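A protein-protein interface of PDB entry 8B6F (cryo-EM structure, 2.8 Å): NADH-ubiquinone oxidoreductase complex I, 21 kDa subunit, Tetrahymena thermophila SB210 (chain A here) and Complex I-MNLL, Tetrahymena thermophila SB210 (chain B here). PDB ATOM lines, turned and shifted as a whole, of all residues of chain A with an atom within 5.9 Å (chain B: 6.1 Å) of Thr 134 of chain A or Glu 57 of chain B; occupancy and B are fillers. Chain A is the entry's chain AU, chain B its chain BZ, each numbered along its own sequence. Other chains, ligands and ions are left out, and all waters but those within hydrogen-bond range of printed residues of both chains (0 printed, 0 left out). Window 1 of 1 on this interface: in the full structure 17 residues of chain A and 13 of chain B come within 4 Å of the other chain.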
ATOM      1  N   ASN A 129     -17.521   5.252 -25.797  1.00  0.00           N
ATOM      2  CA  ASN A 129     -18.278   4.231 -26.507  1.00  0.00           C
ATOM      3  C   ASN A 129     -17.360   3.076 -26.883  1.00  0.00           C
ATOM      4  O   ASN A 129     -17.076   2.853 -28.063  1.00  0.00           O
ATOM      5  CB  ASN A 129     -18.938   4.832 -27.750  1.00  0.00           C
ATOM      6  CG  ASN A 129     -20.033   3.952 -28.313  1.00  0.00           C
ATOM      7  OD1 ASN A 129     -20.568   3.086 -27.622  1.00  0.00           O
ATOM      8  ND2 ASN A 129     -20.376   4.173 -29.577  1.00  0.00           N
ATOM      9  N   TYR A 131     -17.801  -0.242 -26.639  1.00  0.00           N
ATOM     10  CA  TYR A 131     -18.524  -1.268 -27.379  1.00  0.00           C
ATOM     11  C   TYR A 131     -19.581  -0.582 -28.231  1.00  0.00           C
ATOM     12  O   TYR A 131     -20.458   0.107 -27.702  1.00  0.00           O
ATOM     13  CB  TYR A 131     -19.162  -2.275 -26.422  1.00  0.00           C
ATOM     14  CG  TYR A 131     -18.257  -2.665 -25.278  1.00  0.00           C
ATOM     15  CD1 TYR A 131     -17.194  -3.536 -25.473  1.00  0.00           C
ATOM     16  CD2 TYR A 131     -18.465  -2.164 -24.002  1.00  0.00           C
ATOM     17  CE1 TYR A 131     -16.364  -3.893 -24.431  1.00  0.00           C
ATOM     18  CE2 TYR A 131     -17.643  -2.514 -22.956  1.00  0.00           C
ATOM     19  CZ  TYR A 131     -16.594  -3.381 -23.175  1.00  0.00           C
ATOM     20  OH  TYR A 131     -15.770  -3.734 -22.133  1.00  0.00           O
ATOM     21  N   ASP A 132     -19.498  -0.772 -29.546  1.00  0.00           N
ATOM     22  CA  ASP A 132     -20.343  -0.041 -30.490  1.00  0.00           C
ATOM     23  C   ASP A 132     -20.759  -0.995 -31.605  1.00  0.00           C
ATOM     24  O   ASP A 132     -20.021  -1.180 -32.577  1.00  0.00           O
ATOM     25  CB  ASP A 132     -19.606   1.171 -31.043  1.00  0.00           C
ATOM     26  CG  ASP A 132     -20.476   2.023 -31.937  1.00  0.00           C
ATOM     27  OD1 ASP A 132     -21.682   1.723 -32.056  1.00  0.00           O
ATOM     28  OD2 ASP A 132     -19.954   2.992 -32.522  1.00  0.00           O
ATOM     29  N   PHE A 133     -21.937  -1.595 -31.462  1.00  0.00           N
ATOM     30  CA  PHE A 133     -22.509  -2.445 -32.496  1.00  0.00           C
ATOM     31  C   PHE A 133     -23.645  -1.773 -33.256  1.00  0.00           C
ATOM     32  O   PHE A 133     -24.200  -2.383 -34.174  1.00  0.00           O
ATOM     33  CB  PHE A 133     -23.025  -3.750 -31.880  1.00  0.00           C
ATOM     34  CG  PHE A 133     -22.000  -4.491 -31.077  1.00  0.00           C
ATOM     35  CD1 PHE A 133     -21.857  -4.254 -29.720  1.00  0.00           C
ATOM     36  CD2 PHE A 133     -21.189  -5.436 -31.678  1.00  0.00           C
ATOM     37  CE1 PHE A 133     -20.917  -4.941 -28.981  1.00  0.00           C
ATOM     38  CE2 PHE A 133     -20.246  -6.125 -30.943  1.00  0.00           C
ATOM     39  CZ  PHE A 133     -20.112  -5.877 -29.593  1.00  0.00           C
ATOM     40  N   THR A 134     -24.003  -0.538 -32.902  1.00  0.00           N
ATOM     41  CA  THR A 134     -25.202   0.095 -33.432  1.00  0.00           C
ATOM     42  C   THR A 134     -25.001   1.491 -34.003  1.00  0.00           C
ATOM     43  O   THR A 134     -25.933   2.013 -34.623  1.00  0.00           O
ATOM     44  CB  THR A 134     -26.283   0.166 -32.344  1.00  0.00           C
ATOM     45  OG1 THR A 134     -25.729   0.748 -31.163  1.00  0.00           O
ATOM     46  CG2 THR A 134     -26.816  -1.211 -32.020  1.00  0.00           C
ATOM     47  N   SER A 135     -23.832   2.113 -33.831  1.00  0.00           N
ATOM     48  CA  SER A 135     -23.661   3.480 -34.314  1.00  0.00           C
ATOM     49  C   SER A 135     -23.808   3.538 -35.828  1.00  0.00           C
ATOM     50  O   SER A 135     -24.599   4.327 -36.357  1.00  0.00           O
ATOM     51  CB  SER A 135     -22.301   4.029 -33.882  1.00  0.00           C
ATOM     52  OG  SER A 135     -21.244   3.272 -34.445  1.00  0.00           O
ATOM     53  N   GLU A 136     -23.046   2.713 -36.547  1.00  0.00           N
ATOM     54  CA  GLU A 136     -23.138   2.713 -38.003  1.00  0.00           C
ATOM     55  C   GLU A 136     -24.507   2.224 -38.461  1.00  0.00           C
ATOM     56  O   GLU A 136     -25.071   2.753 -39.424  1.00  0.00           O
ATOM     57  CB  GLU A 136     -22.025   1.852 -38.606  1.00  0.00           C
ATOM     58  CG  GLU A 136     -22.234   0.342 -38.501  1.00  0.00           C
ATOM     59  CD  GLU A 136     -22.309  -0.153 -37.067  1.00  0.00           C
ATOM     60  OE1 GLU A 136     -21.917   0.602 -36.152  1.00  0.00           O
ATOM     61  OE2 GLU A 136     -22.761  -1.299 -36.854  1.00  0.00           O
ATOM     62  N   PHE A 137     -25.051   1.209 -37.787  1.00  0.00           N
ATOM     63  CA  PHE A 137     -26.357   0.679 -38.161  1.00  0.00           C
ATOM     64  C   PHE A 137     -27.430   1.755 -38.056  1.00  0.00           C
ATOM     65  O   PHE A 137     -28.236   1.937 -38.974  1.00  0.00           O
ATOM     66  CB  PHE A 137     -26.702  -0.518 -37.274  1.00  0.00           C
ATOM     67  CG  PHE A 137     -28.003  -1.181 -37.627  1.00  0.00           C
ATOM     68  CD1 PHE A 137     -28.044  -2.205 -38.557  1.00  0.00           C
ATOM     69  CD2 PHE A 137     -29.184  -0.788 -37.020  1.00  0.00           C
ATOM     70  CE1 PHE A 137     -29.236  -2.819 -38.882  1.00  0.00           C
ATOM     71  CE2 PHE A 137     -30.380  -1.398 -37.339  1.00  0.00           C
ATOM     72  CZ  PHE A 137     -30.406  -2.414 -38.270  1.00  0.00           C
ATOM     73  N   GLU A 138     -27.447   2.487 -36.940  1.00  0.00           N
ATOM     74  CA  GLU A 138     -28.417   3.565 -36.772  1.00  0.00           C
ATOM     75  C   GLU A 138     -28.187   4.687 -37.776  1.00  0.00           C
ATOM     76  O   GLU A 138     -29.141   5.209 -38.360  1.00  0.00           O
ATOM     77  CB  GLU A 138     -28.356   4.106 -35.346  1.00  0.00           C
ATOM     78  CG  GLU A 138     -28.837   3.124 -34.296  1.00  0.00           C
ATOM     79  CD  GLU A 138     -28.689   3.664 -32.889  1.00  0.00           C
ATOM     80  OE1 GLU A 138     -28.027   4.708 -32.721  1.00  0.00           O
ATOM     81  OE2 GLU A 138     -29.239   3.049 -31.953  1.00  0.00           O
ATOM     82  N   ASP A 139     -26.927   5.069 -37.995  1.00  0.00           N
ATOM     83  CA  ASP A 139     -26.642   6.157 -38.924  1.00  0.00           C
ATOM     84  C   ASP A 139     -27.124   5.822 -40.327  1.00  0.00           C
ATOM     85  O   ASP A 139     -27.613   6.698 -41.050  1.00  0.00           O
ATOM     86  CB  ASP A 139     -25.145   6.464 -38.933  1.00  0.00           C
ATOM     87  CG  ASP A 139     -24.645   6.980 -37.595  1.00  0.00           C
ATOM     88  OD1 ASP A 139     -25.463   7.103 -36.659  1.00  0.00           O
ATOM     89  OD2 ASP A 139     -23.433   7.262 -37.479  1.00  0.00           O
ATOM     90  N   ARG A 147     -33.053   6.535 -30.746  1.00  0.00           N
ATOM     91  CA  ARG A 147     -32.005   6.526 -29.738  1.00  0.00           C
ATOM     92  C   ARG A 147     -31.458   7.929 -29.527  1.00  0.00           C
ATOM     93  O   ARG A 147     -31.374   8.732 -30.459  1.00  0.00           O
ATOM     94  CB  ARG A 147     -30.864   5.582 -30.126  1.00  0.00           C
ATOM     95  CG  ARG A 147     -29.856   5.398 -29.010  1.00  0.00           C
ATOM     96  CD  ARG A 147     -28.903   4.259 -29.286  1.00  0.00           C
ATOM     97  NE  ARG A 147     -28.091   3.955 -28.116  1.00  0.00           N
ATOM     98  CZ  ARG A 147     -27.182   2.993 -28.066  1.00  0.00           C
ATOM     99  NH1 ARG A 147     -26.936   2.225 -29.108  1.00  0.00           N
ATOM    100  NH2 ARG A 147     -26.501   2.797 -26.942  1.00  0.00           N
ATOM    101  N   ARG A 149     -28.163  10.040 -28.194  1.00  0.00           N
ATOM    102  CA  ARG A 149     -26.726   9.947 -27.986  1.00  0.00           C
ATOM    103  C   ARG A 149     -26.194  11.283 -27.489  1.00  0.00           C
ATOM    104  O   ARG A 149     -26.560  12.342 -28.010  1.00  0.00           O
ATOM    105  CB  ARG A 149     -26.007   9.541 -29.275  1.00  0.00           C
ATOM    106  CG  ARG A 149     -26.347   8.136 -29.743  1.00  0.00           C
ATOM    107  CD  ARG A 149     -25.517   7.733 -30.950  1.00  0.00           C
ATOM    108  NE  ARG A 149     -25.739   6.340 -31.317  1.00  0.00           N
ATOM    109  CZ  ARG A 149     -25.107   5.309 -30.775  1.00  0.00           C
ATOM    110  NH1 ARG A 149     -24.200   5.472 -29.825  1.00  0.00           N
ATOM    111  NH2 ARG A 149     -25.393   4.079 -31.193  1.00  0.00           N
ATOM    112  N   TRP B  50     -32.028  -4.381 -35.036  1.00  0.00           N
ATOM    113  CA  TRP B  50     -31.561  -3.271 -34.213  1.00  0.00           C
ATOM    114  C   TRP B  50     -31.523  -3.662 -32.743  1.00  0.00           C
ATOM    115  O   TRP B  50     -30.566  -3.343 -32.029  1.00  0.00           O
ATOM    116  CB  TRP B  50     -32.463  -2.057 -34.425  1.00  0.00           C
ATOM    117  CG  TRP B  50     -32.045  -0.840 -33.664  1.00  0.00           C
ATOM    118  CD1 TRP B  50     -30.846  -0.198 -33.743  1.00  0.00           C
ATOM    119  CD2 TRP B  50     -32.836  -0.101 -32.727  1.00  0.00           C
ATOM    120  NE1 TRP B  50     -30.837   0.891 -32.908  1.00  0.00           N
ATOM    121  CE2 TRP B  50     -32.045   0.970 -32.268  1.00  0.00           C
ATOM    122  CE3 TRP B  50     -34.132  -0.246 -32.224  1.00  0.00           C
ATOM    123  CZ2 TRP B  50     -32.510   1.896 -31.340  1.00  0.00           C
ATOM    124  CZ3 TRP B  50     -34.592   0.672 -31.299  1.00  0.00           C
ATOM    125  CH2 TRP B  50     -33.782   1.730 -30.866  1.00  0.00           C
ATOM    126  N   ARG B  52     -31.250  -6.614 -31.222  1.00  0.00           N
ATOM    127  CA  ARG B  52     -30.221  -7.568 -30.821  1.00  0.00           C
ATOM    128  C   ARG B  52     -28.882  -6.873 -30.624  1.00  0.00           C
ATOM    129  O   ARG B  52     -28.148  -7.180 -29.679  1.00  0.00           O
ATOM    130  CB  ARG B  52     -30.097  -8.696 -31.848  1.00  0.00           C
ATOM    131  CG  ARG B  52     -29.632  -8.266 -33.231  1.00  0.00           C
ATOM    132  CD  ARG B  52     -29.221  -9.467 -34.064  1.00  0.00           C
ATOM    133  NE  ARG B  52     -28.642  -9.065 -35.338  1.00  0.00           N
ATOM    134  CZ  ARG B  52     -28.066  -9.897 -36.195  1.00  0.00           C
ATOM    135  NH1 ARG B  52     -27.960 -11.189 -35.938  1.00  0.00           N
ATOM    136  NH2 ARG B  52     -27.582  -9.420 -37.337  1.00  0.00           N
ATOM    137  N   ARG B  53     -28.539  -5.935 -31.508  1.00  0.00           N
ATOM    138  CA  ARG B  53     -27.275  -5.225 -31.362  1.00  0.00           C
ATOM    139  C   ARG B  53     -27.298  -4.303 -30.148  1.00  0.00           C
ATOM    140  O   ARG B  53     -26.297  -4.192 -29.432  1.00  0.00           O
ATOM    141  CB  ARG B  53     -26.971  -4.445 -32.638  1.00  0.00           C
ATOM    142  CG  ARG B  53     -26.951  -5.324 -33.876  1.00  0.00           C
ATOM    143  CD  ARG B  53     -26.370  -4.611 -35.078  1.00  0.00           C
ATOM    144  NE  ARG B  53     -26.404  -5.461 -36.260  1.00  0.00           N
ATOM    145  CZ  ARG B  53     -25.721  -5.230 -37.373  1.00  0.00           C
ATOM    146  NH1 ARG B  53     -24.922  -4.182 -37.488  1.00  0.00           N
ATOM    147  NH2 ARG B  53     -25.836  -6.074 -38.392  1.00  0.00           N
ATOM    148  N   MET B  54     -28.421  -3.628 -29.902  1.00  0.00           N
ATOM    149  CA  MET B  54     -28.524  -2.809 -28.697  1.00  0.00           C
ATOM    150  C   MET B  54     -28.384  -3.662 -27.446  1.00  0.00           C
ATOM    151  O   MET B  54     -27.705  -3.272 -26.490  1.00  0.00           O
ATOM    152  CB  MET B  54     -29.851  -2.055 -28.673  1.00  0.00           C
ATOM    153  CG  MET B  54     -29.811  -0.719 -29.384  1.00  0.00           C
ATOM    154  SD  MET B  54     -31.200   0.332 -28.934  1.00  0.00           S
ATOM    155  CE  MET B  54     -30.824   0.707 -27.228  1.00  0.00           C
ATOM    156  N   ALA B  55     -29.035  -4.826 -27.427  1.00  0.00           N
ATOM    157  CA  ALA B  55     -28.929  -5.715 -26.278  1.00  0.00           C
ATOM    158  C   ALA B  55     -27.499  -6.205 -26.095  1.00  0.00           C
ATOM    159  O   ALA B  55     -27.005  -6.296 -24.967  1.00  0.00           O
ATOM    160  CB  ALA B  55     -29.882  -6.898 -26.443  1.00  0.00           C
ATOM    161  N   LEU B  56     -26.820  -6.526 -27.197  1.00  0.00           N
ATOM    162  CA  LEU B  56     -25.434  -6.967 -27.106  1.00  0.00           C
ATOM    163  C   LEU B  56     -24.544  -5.869 -26.543  1.00  0.00           C
ATOM    164  O   LEU B  56     -23.685  -6.132 -25.694  1.00  0.00           O
ATOM    165  CB  LEU B  56     -24.936  -7.404 -28.483  1.00  0.00           C
ATOM    166  CG  LEU B  56     -23.501  -7.929 -28.552  1.00  0.00           C
ATOM    167  CD1 LEU B  56     -23.321  -9.148 -27.663  1.00  0.00           C
ATOM    168  CD2 LEU B  56     -23.129  -8.252 -29.986  1.00  0.00           C
ATOM    169  N   GLU B  57     -24.731  -4.631 -27.000  1.00  0.00           N
ATOM    170  CA  GLU B  57     -23.927  -3.528 -26.487  1.00  0.00           C
ATOM    171  C   GLU B  57     -24.172  -3.322 -24.997  1.00  0.00           C
ATOM    172  O   GLU B  57     -23.227  -3.156 -24.219  1.00  0.00           O
ATOM    173  CB  GLU B  57     -24.239  -2.254 -27.271  1.00  0.00           C
ATOM    174  CG  GLU B  57     -23.416  -1.054 -26.855  1.00  0.00           C
ATOM    175  CD  GLU B  57     -23.688   0.155 -27.725  1.00  0.00           C
ATOM    176  OE1 GLU B  57     -24.516   0.043 -28.653  1.00  0.00           O
ATOM    177  OE2 GLU B  57     -23.078   1.216 -27.482  1.00  0.00           O
ATOM    178  N   GLN B  58     -25.439  -3.332 -24.580  1.00  0.00           N
ATOM    179  CA  GLN B  58     -25.747  -3.136 -23.168  1.00  0.00           C
ATOM    180  C   GLN B  58     -25.253  -4.303 -22.325  1.00  0.00           C
ATOM    181  O   GLN B  58     -24.848  -4.109 -21.175  1.00  0.00           O
ATOM    182  CB  GLN B  58     -27.247  -2.936 -22.969  1.00  0.00           C
ATOM    183  CG  GLN B  58     -27.638  -2.632 -21.530  1.00  0.00           C
ATOM    184  CD  GLN B  58     -26.898  -1.440 -20.963  1.00  0.00           C
ATOM    185  OE1 GLN B  58     -26.523  -0.523 -21.689  1.00  0.00           O
ATOM    186  NE2 GLN B  58     -26.675  -1.452 -19.653  1.00  0.00           N
ATOM    187  N   LEU B  59     -25.281  -5.515 -22.878  1.00  0.00           N
ATOM    188  CA  LEU B  59     -24.728  -6.663 -22.168  1.00  0.00           C
ATOM    189  C   LEU B  59     -23.226  -6.523 -21.990  1.00  0.00           C
ATOM    190  O   LEU B  59     -22.694  -6.823 -20.916  1.00  0.00           O
ATOM    191  CB  LEU B  59     -25.066  -7.948 -22.919  1.00  0.00           C
ATOM    192  CG  LEU B  59     -24.345  -9.222 -22.476  1.00  0.00           C
ATOM    193  CD1 LEU B  59     -24.540  -9.487 -20.992  1.00  0.00           C
ATOM    194  CD2 LEU B  59     -24.847 -10.393 -23.295  1.00  0.00           C
ATOM    195  N   CYS B  60     -22.524  -6.057 -23.022  1.00  0.00           N
ATOM    196  CA  CYS B  60     -21.092  -5.824 -22.885  1.00  0.00           C
ATOM    197  C   CYS B  60     -20.808  -4.794 -21.801  1.00  0.00           C
ATOM    198  O   CYS B  60     -19.861  -4.946 -21.021  1.00  0.00           O
ATOM    199  CB  CYS B  60     -20.508  -5.370 -24.221  1.00  0.00           C
ATOM    200  SG  CYS B  60     -20.409  -6.671 -25.467  1.00  0.00           S
ATOM    201  N   TYR B  61     -21.610  -3.731 -21.740  1.00  0.00           N
ATOM    202  CA  TYR B  61     -21.433  -2.733 -20.690  1.00  0.00           C
ATOM    203  C   TYR B  61     -21.753  -3.312 -19.317  1.00  0.00           C
ATOM    204  O   TYR B  61     -21.067  -3.008 -18.335  1.00  0.00           O
ATOM    205  CB  TYR B  61     -22.304  -1.512 -20.978  1.00  0.00           C
ATOM    206  CG  TYR B  61     -21.711  -0.586 -22.013  1.00  0.00           C
ATOM    207  CD1 TYR B  61     -20.630   0.229 -21.709  1.00  0.00           C
ATOM    208  CD2 TYR B  61     -22.236  -0.526 -23.296  1.00  0.00           C
ATOM    209  CE1 TYR B  61     -20.086   1.074 -22.655  1.00  0.00           C
ATOM    210  CE2 TYR B  61     -21.701   0.315 -24.247  1.00  0.00           C
ATOM    211  CZ  TYR B  61     -20.627   1.113 -23.922  1.00  0.00           C
ATOM    212  OH  TYR B  61     -20.095   1.952 -24.871  1.00  0.00           O
ATOM    213  N   ASN B  62     -22.799  -4.137 -19.223  1.00  0.00           N
ATOM    214  CA  ASN B  62     -23.159  -4.720 -17.934  1.00  0.00           C
ATOM    215  C   ASN B  62     -22.085  -5.671 -17.426  1.00  0.00           C
ATOM    216  O   ASN B  62     -21.891  -5.789 -16.211  1.00  0.00           O
ATOM    217  CB  ASN B  62     -24.490  -5.463 -18.040  1.00  0.00           C
ATOM    218  CG  ASN B  62     -25.663  -4.534 -18.240  1.00  0.00           C
ATOM    219  OD1 ASN B  62     -25.578  -3.338 -17.965  1.00  0.00           O
ATOM    220  ND2 ASN B  62     -26.774  -5.083 -18.714  1.00  0.00           N
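OD1 of Asn 129 of chain A lies close to OE2 of Glu 57 of chain B.
The side-chain amide oxygen (OD1) of Asn 129 of chain A is in hydrogen-bond range of the side-chain hydroxyl (OH) of Tyr 61 of chain B, 3.0 Å away.
O of Tyr 131 of chain A sits at hydrogen-bond distance from OH of Tyr 61 of chain B.
The side-chain carboxylate (OE1) of Glu 57 of chain B is in hydrogen-bond range of the side-chain hydroxyl (OG1) of Thr 134 of chain A (2.9 Å).
The guanidinium group of Arg 53 of chain B is in salt-bridge range of the side-chain carboxylate of Glu 136 of chain A (3.7 Å).
The side-chain carboxylate (OE2) of Glu 138 of chain A lies within hydrogen-bond range of the indole nitrogen (NE1) of Trp 50 of chain B, at 2.9 Å.
The guanidinium group (NH1) of Arg 147 of chain A lies within salt-bridge range of the side-chain carboxylate (OE1) of Glu 57 of chain B, at 3.3 Å.
The side-chain carboxylate (OE2) of Glu 57 of chain B sits close to the backbone carbonyl oxygen (O) of Tyr 131 of chain A (2.9 Å).
OD2 of Asp 132 of chain A sits close to ND2 of Asn 129 of chain A, at 3.2 Å.
The side-chain hydroxyl of Thr 134 of chain A lies within hydrogen-bond range of the guanidinium group of Arg 147 of chain A, at 2.8 Å.
OG1 of Thr 134 of chain A lies within hydrogen-bond range of NH2 of Arg 149 of chain A (3.3 Å).
The side-chain hydroxyl of Ser 135 of chain A lies within hydrogen-bond range of the side-chain carboxylate of Glu 136 of chain A (3.2 Å).
The side-chain carboxylate (OE1) of Glu 138 of chain A is in salt-bridge range of the guanidinium group (NH2) of Arg 149 of chain A (3.1 Å).
The backbone carbonyl oxygen (O) of Leu 56 of chain B is in hydrogen-bond range of the side-chain sulfur (SG) of Cys 60 of chain B, 3.3 Å away.
Among the printed residues, pairs that only touch across the chains: Phe 133 of chain A with Arg 53 of chain B (3.2 Å), Thr 134 of chain A with Arg 53 of chain B (3.3 Å), Thr 134 of chain A with Met 54 of chain B (3.6 Å), Phe 137 of chain A with Trp 50 of chain B (3.6 Å), Tyr 131 of chain A with Cys 60 of chain B (3.7 Å), Phe 133 of chain A with Leu 56 of chain B (3.7 Å), Phe 137 of chain A with Arg 53 of chain B (3.8 Å), Phe 133 of chain A with Glu 57 of chain B (3.9 Å) and Phe 133 of chain A with Cys 60 of chain B (3.9 Å).
Of the printed residues of chain B, Thr 134 of chain A touches Arg 53 (3.3 Å), Met 54 (3.6 Å) and Glu 57 (2.9 Å).
Glu 57 of chain B touches just these residues of chain A: Asn 129 (3.1 Å), Tyr 131 (2.9 Å), Phe 133 (3.9 Å), Thr 134 (2.9 Å) and Arg 147 (3.3 Å).
Printed residues of chain B within 4 Å of Glu 138 of chain A: Trp 50 (2.9 Å).
Of the printed residues of chain A, Met 54 of chain B touches Thr 134.
Ala 55 of chain B touches none of the printed residues of chain A.
Arg 52 of chain B touches none of the printed residues of chain A.
The nearest residue of chain B that does not touch Thr 134 of chain A is Trp 50 of chain B (4.3 Å).
The nearest residue of chain A that does not touch Glu 57 of chain B is Asp 132 of chain A (4.3 Å).
Of the 12 printed residues of chain B, 7 touch a printed residue of chain A.
Printed residues of chain B that touch a printed residue of chain A: Trp 50, Arg 53, Met 54, Leu 56, Glu 57, Cys 60 and Tyr 61.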
